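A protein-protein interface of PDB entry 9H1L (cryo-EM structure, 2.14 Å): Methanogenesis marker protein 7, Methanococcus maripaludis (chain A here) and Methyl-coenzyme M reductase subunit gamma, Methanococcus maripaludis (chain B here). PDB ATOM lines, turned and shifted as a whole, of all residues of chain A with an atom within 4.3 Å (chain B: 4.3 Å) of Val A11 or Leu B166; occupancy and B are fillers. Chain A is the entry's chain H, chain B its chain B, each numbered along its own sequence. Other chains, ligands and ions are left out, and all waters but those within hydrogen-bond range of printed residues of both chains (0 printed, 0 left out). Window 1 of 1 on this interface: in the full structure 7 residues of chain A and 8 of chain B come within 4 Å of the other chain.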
ATOM      1  N   GLY A  10      -5.848  15.636  -6.703  1.00  0.00           N
ATOM      2  CA  GLY A  10      -6.571  14.400  -6.942  1.00  0.00           C
ATOM      3  C   GLY A  10      -7.046  13.741  -5.666  1.00  0.00           C
ATOM      4  O   GLY A  10      -6.585  14.086  -4.576  1.00  0.00           O
ATOM      5  N   VAL A  11      -7.972  12.790  -5.787  1.00  0.00           N
ATOM      6  CA  VAL A  11      -8.462  12.083  -4.609  1.00  0.00           C
ATOM      7  C   VAL A  11      -7.475  11.035  -4.117  1.00  0.00           C
ATOM      8  O   VAL A  11      -7.582  10.592  -2.967  1.00  0.00           O
ATOM      9  CB  VAL A  11      -9.820  11.419  -4.881  1.00  0.00           C
ATOM     10  CG1 VAL A  11     -10.894  12.472  -5.043  1.00  0.00           C
ATOM     11  CG2 VAL A  11      -9.743  10.529  -6.109  1.00  0.00           C
ATOM     12  N   TYR A  12      -6.529  10.619  -4.954  1.00  0.00           N
ATOM     13  CA  TYR A  12      -5.526   9.653  -4.533  1.00  0.00           C
ATOM     14  C   TYR A  12      -4.570  10.296  -3.537  1.00  0.00           C
ATOM     15  O   TYR A  12      -4.005  11.361  -3.809  1.00  0.00           O
ATOM     16  CB  TYR A  12      -4.760   9.124  -5.741  1.00  0.00           C
ATOM     17  CG  TYR A  12      -3.746   8.056  -5.410  1.00  0.00           C
ATOM     18  CD1 TYR A  12      -4.069   7.003  -4.567  1.00  0.00           C
ATOM     19  CD2 TYR A  12      -2.467   8.101  -5.944  1.00  0.00           C
ATOM     20  CE1 TYR A  12      -3.143   6.027  -4.262  1.00  0.00           C
ATOM     21  CE2 TYR A  12      -1.535   7.129  -5.644  1.00  0.00           C
ATOM     22  CZ  TYR A  12      -1.879   6.094  -4.803  1.00  0.00           C
ATOM     23  OH  TYR A  12      -0.956   5.121  -4.502  1.00  0.00           O
ATOM     24  N   LYS A  13      -4.418   9.652  -2.374  1.00  0.00           N
ATOM     25  CA  LYS A  13      -3.589  10.127  -1.258  1.00  0.00           C
ATOM     26  C   LYS A  13      -4.024  11.504  -0.757  1.00  0.00           C
ATOM     27  O   LYS A  13      -3.223  12.251  -0.192  1.00  0.00           O
ATOM     28  CB  LYS A  13      -2.102  10.131  -1.621  1.00  0.00           C
ATOM     29  CG  LYS A  13      -1.592   8.814  -2.170  1.00  0.00           C
ATOM     30  CD  LYS A  13      -0.168   8.544  -1.721  1.00  0.00           C
ATOM     31  CE  LYS A  13       0.812   8.703  -2.869  1.00  0.00           C
ATOM     32  NZ  LYS A  13       1.255   7.389  -3.410  1.00  0.00           N
ATOM     33  N   ASN A  14      -5.297  11.851  -0.958  1.00  0.00           N
ATOM     34  CA  ASN A  14      -5.817  13.112  -0.444  1.00  0.00           C
ATOM     35  C   ASN A  14      -6.056  13.052   1.056  1.00  0.00           C
ATOM     36  O   ASN A  14      -5.972  14.081   1.736  1.00  0.00           O
ATOM     37  CB  ASN A  14      -7.109  13.483  -1.168  1.00  0.00           C
ATOM     38  CG  ASN A  14      -7.580  14.884  -0.836  1.00  0.00           C
ATOM     39  OD1 ASN A  14      -6.825  15.849  -0.949  1.00  0.00           O
ATOM     40  ND2 ASN A  14      -8.834  15.004  -0.419  1.00  0.00           N
ATOM     41  N   VAL A  33     -15.694  16.503  -4.209  1.00  0.00           N
ATOM     42  CA  VAL A  33     -15.054  15.540  -5.097  1.00  0.00           C
ATOM     43  C   VAL A  33     -15.941  15.389  -6.323  1.00  0.00           C
ATOM     44  O   VAL A  33     -17.110  15.000  -6.203  1.00  0.00           O
ATOM     45  CB  VAL A  33     -14.842  14.187  -4.401  1.00  0.00           C
ATOM     46  CG1 VAL A  33     -14.512  13.108  -5.419  1.00  0.00           C
ATOM     47  CG2 VAL A  33     -13.749  14.296  -3.352  1.00  0.00           C
ATOM     48  N   LEU A  36     -12.547  12.423  -9.936  1.00  0.00           N
ATOM     49  CA  LEU A  36     -11.253  12.002  -9.420  1.00  0.00           C
ATOM     50  C   LEU A  36     -10.439  13.170  -8.890  1.00  0.00           C
ATOM     51  O   LEU A  36      -9.354  12.947  -8.349  1.00  0.00           O
ATOM     52  CB  LEU A  36     -10.439  11.275 -10.505  1.00  0.00           C
ATOM     53  CG  LEU A  36     -10.939   9.917 -10.997  1.00  0.00           C
ATOM     54  CD1 LEU A  36     -10.481   9.676 -12.425  1.00  0.00           C
ATOM     55  CD2 LEU A  36     -10.454   8.803 -10.086  1.00  0.00           C
ATOM     56  N   VAL A  38     -10.421  16.773  -6.417  1.00  0.00           N
ATOM     57  CA  VAL A  38     -11.057  17.316  -5.225  1.00  0.00           C
ATOM     58  C   VAL A  38     -10.719  18.798  -5.123  1.00  0.00           C
ATOM     59  O   VAL A  38      -9.565  19.195  -5.327  1.00  0.00           O
ATOM     60  CB  VAL A  38     -10.638  16.536  -3.960  1.00  0.00           C
ATOM     61  CG1 VAL A  38      -9.121  16.411  -3.849  1.00  0.00           C
ATOM     62  CG2 VAL A  38     -11.225  17.163  -2.703  1.00  0.00           C
ATOM     63  N   SER B  93      -3.454   0.317 -15.863  1.00  0.00           N
ATOM     64  CA  SER B  93      -3.236   1.731 -15.601  1.00  0.00           C
ATOM     65  C   SER B  93      -1.815   2.135 -15.976  1.00  0.00           C
ATOM     66  O   SER B  93      -0.868   1.356 -15.859  1.00  0.00           O
ATOM     67  CB  SER B  93      -3.501   2.044 -14.130  1.00  0.00           C
ATOM     68  OG  SER B  93      -3.154   3.378 -13.818  1.00  0.00           O
ATOM     69  N   LEU B 164      -6.275   7.695 -16.649  1.00  0.00           N
ATOM     70  CA  LEU B 164      -6.762   8.554 -15.584  1.00  0.00           C
ATOM     71  C   LEU B 164      -6.016   8.273 -14.283  1.00  0.00           C
ATOM     72  O   LEU B 164      -5.357   7.244 -14.122  1.00  0.00           O
ATOM     73  CB  LEU B 164      -8.263   8.364 -15.372  1.00  0.00           C
ATOM     74  CG  LEU B 164      -9.172   8.510 -16.591  1.00  0.00           C
ATOM     75  CD1 LEU B 164     -10.625   8.334 -16.187  1.00  0.00           C
ATOM     76  CD2 LEU B 164      -8.959   9.855 -17.261  1.00  0.00           C
ATOM     77  N   ARG B 165      -6.131   9.213 -13.350  1.00  0.00           N
ATOM     78  CA  ARG B 165      -5.523   9.048 -12.040  1.00  0.00           C
ATOM     79  C   ARG B 165      -6.296   8.019 -11.218  1.00  0.00           C
ATOM     80  O   ARG B 165      -7.473   7.743 -11.458  1.00  0.00           O
ATOM     81  CB  ARG B 165      -5.481  10.381 -11.297  1.00  0.00           C
ATOM     82  CG  ARG B 165      -4.474  11.370 -11.850  1.00  0.00           C
ATOM     83  CD  ARG B 165      -4.774  12.776 -11.366  1.00  0.00           C
ATOM     84  NE  ARG B 165      -6.092  13.225 -11.789  1.00  0.00           N
ATOM     85  CZ  ARG B 165      -6.637  14.380 -11.436  1.00  0.00           C
ATOM     86  NH1 ARG B 165      -6.002  15.234 -10.651  1.00  0.00           N
ATOM     87  NH2 ARG B 165      -7.852  14.687 -11.883  1.00  0.00           N
ATOM     88  N   LEU B 166      -5.605   7.445 -10.236  1.00  0.00           N
ATOM     89  CA  LEU B 166      -6.226   6.470  -9.354  1.00  0.00           C
ATOM     90  C   LEU B 166      -7.191   7.156  -8.393  1.00  0.00           C
ATOM     91  O   LEU B 166      -7.140   8.369  -8.173  1.00  0.00           O
ATOM     92  CB  LEU B 166      -5.161   5.704  -8.575  1.00  0.00           C
ATOM     93  CG  LEU B 166      -4.008   5.135  -9.407  1.00  0.00           C
ATOM     94  CD1 LEU B 166      -2.921   4.581  -8.507  1.00  0.00           C
ATOM     95  CD2 LEU B 166      -4.512   4.067 -10.358  1.00  0.00           C
ATOM     96  N   ASP B 167      -8.088   6.360  -7.815  1.00  0.00           N
ATOM     97  CA  ASP B 167      -9.075   6.885  -6.883  1.00  0.00           C
ATOM     98  C   ASP B 167      -8.458   6.999  -5.487  1.00  0.00           C
ATOM     99  O   ASP B 167      -7.244   6.882  -5.304  1.00  0.00           O
ATOM    100  CB  ASP B 167     -10.340   6.027  -6.901  1.00  0.00           C
ATOM    101  CG  ASP B 167     -10.096   4.589  -6.469  1.00  0.00           C
ATOM    102  OD1 ASP B 167      -8.929   4.173  -6.329  1.00  0.00           O
ATOM    103  OD2 ASP B 167     -11.092   3.863  -6.264  1.00  0.00           O
ATOM    104  N   GLU B 168      -9.304   7.223  -4.480  1.00  0.00           N
ATOM    105  CA  GLU B 168      -8.826   7.388  -3.112  1.00  0.00           C
ATOM    106  C   GLU B 168      -8.266   6.100  -2.521  1.00  0.00           C
ATOM    107  O   GLU B 168      -7.516   6.161  -1.543  1.00  0.00           O
ATOM    108  CB  GLU B 168      -9.952   7.922  -2.223  1.00  0.00           C
ATOM    109  CG  GLU B 168     -11.062   6.925  -1.927  1.00  0.00           C
ATOM    110  CD  GLU B 168     -12.081   6.828  -3.046  1.00  0.00           C
ATOM    111  OE1 GLU B 168     -12.173   7.780  -3.850  1.00  0.00           O
ATOM    112  OE2 GLU B 168     -12.790   5.803  -3.124  1.00  0.00           O
ATOM    113  N   GLY B 170      -6.504   3.911  -4.477  1.00  0.00           N
ATOM    114  CA  GLY B 170      -5.430   3.487  -5.349  1.00  0.00           C
ATOM    115  C   GLY B 170      -5.837   2.578  -6.483  1.00  0.00           C
ATOM    116  O   GLY B 170      -4.962   1.990  -7.128  1.00  0.00           O
ATOM    117  N   MET B 171      -7.128   2.440  -6.751  1.00  0.00           N
ATOM    118  CA  MET B 171      -7.631   1.571  -7.799  1.00  0.00           C
ATOM    119  C   MET B 171      -7.843   2.354  -9.090  1.00  0.00           C
ATOM    120  O   MET B 171      -8.030   3.572  -9.082  1.00  0.00           O
ATOM    121  CB  MET B 171      -8.945   0.914  -7.368  1.00  0.00           C
ATOM    122  CG  MET B 171      -8.794  -0.110  -6.262  1.00  0.00           C
ATOM    123  SD  MET B 171     -10.304  -0.295  -5.300  1.00  0.00           S
ATOM    124  CE  MET B 171     -11.296  -1.283  -6.411  1.00  0.00           C
ATOM    125  N   MET B 172      -7.801   1.633 -10.205  1.00  0.00           N
ATOM    126  CA  MET B 172      -8.084   2.240 -11.495  1.00  0.00           C
ATOM    127  C   MET B 172      -9.562   2.608 -11.581  1.00  0.00           C
ATOM    128  O   MET B 172     -10.423   1.942 -11.000  1.00  0.00           O
ATOM    129  CB  MET B 172      -7.713   1.282 -12.628  1.00  0.00           C
ATOM    130  CG  MET B 172      -7.731   1.911 -14.016  1.00  0.00           C
ATOM    131  SD  MET B 172      -7.316   0.821 -15.392  1.00  0.00           S
ATOM    132  CE  MET B 172      -7.187  -0.759 -14.572  1.00  0.00           C
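The backbone NH of Gly B170 sits at hydrogen-bond distance from the side-chain carboxylate of Asp B167 (3.1 Å). The side-chain carboxylate of Asp B167 lies within hydrogen-bond range of the backbone NH of Met B171 (2.5 Å). N of Val A11 sits at hydrogen-bond distance from O of Leu A36 (2.9 Å). The side-chain amino group of Lys A13 sits at hydrogen-bond distance from the side-chain hydroxyl of Tyr A12 (3.4 Å).
Gly A10 touches Arg B165 (CA to NH1, 3.8 Å). Val A11 touches Leu B166 (CG2 to O, 3.96 Å). CA of Glu B168 touches O of Val A11, at 3.4 Å. Tyr A12 touches Leu B166. Asp B167 touches Tyr A12. CE1 of Tyr A12 touches CA of Gly B170, at 3.6 Å. CB of Leu B164 touches CD1 of Leu A36, 3.9 Å away. O of Arg B165 touches CD2 of Leu A36, at 3.4 Å. Leu A36 touches Leu B166. Asp B167 touches Leu A36.
Val A11 touches just these residues of chain B: Leu B166 (3.96 Å), Asp B167 (3.8 Å) and Glu B168 (3.4 Å). Leu B166 touches three residues of chain A. Printed residues of chain A within 4 Å of Asp B167: Val A11 (3.8 Å), Tyr A12 (3.3 Å) and Leu A36 (3.98 Å). Printed residues of chain A within 4 Å of Arg B165: Gly A10 and Leu A36. Of the printed residues of chain B, Leu A36 touches Leu B164 (3.9 Å), Arg B165 (3.4 Å), Leu B166 (3.9 Å) and Asp B167 (3.98 Å). Printed residues of chain A within 4 Å of Leu B164: Leu A36 (3.9 Å). Val A33 touches none of the printed residues of chain B. Asn A14 touches none of the printed residues of chain B. The nearest printed residue of chain B that does not touch Val A11 is Arg B165 (5.8 Å).
Of the 9 printed residues of chain B, 6 touch a printed residue of chain A. Of the 8 printed residues of chain A, 4 touch a printed residue of chain B. Hydrophobic or aromatic side chains of chain A within 4 Å of the printed part of chain B: Val A11, Tyr A12 and Leu A36. Among the printed residues, 11 pairs touch across the chains. Among the printed residues, no Asp or Glu carboxylate lies within 4 Å of a Lys or Arg side-chain nitrogen of the other chain.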
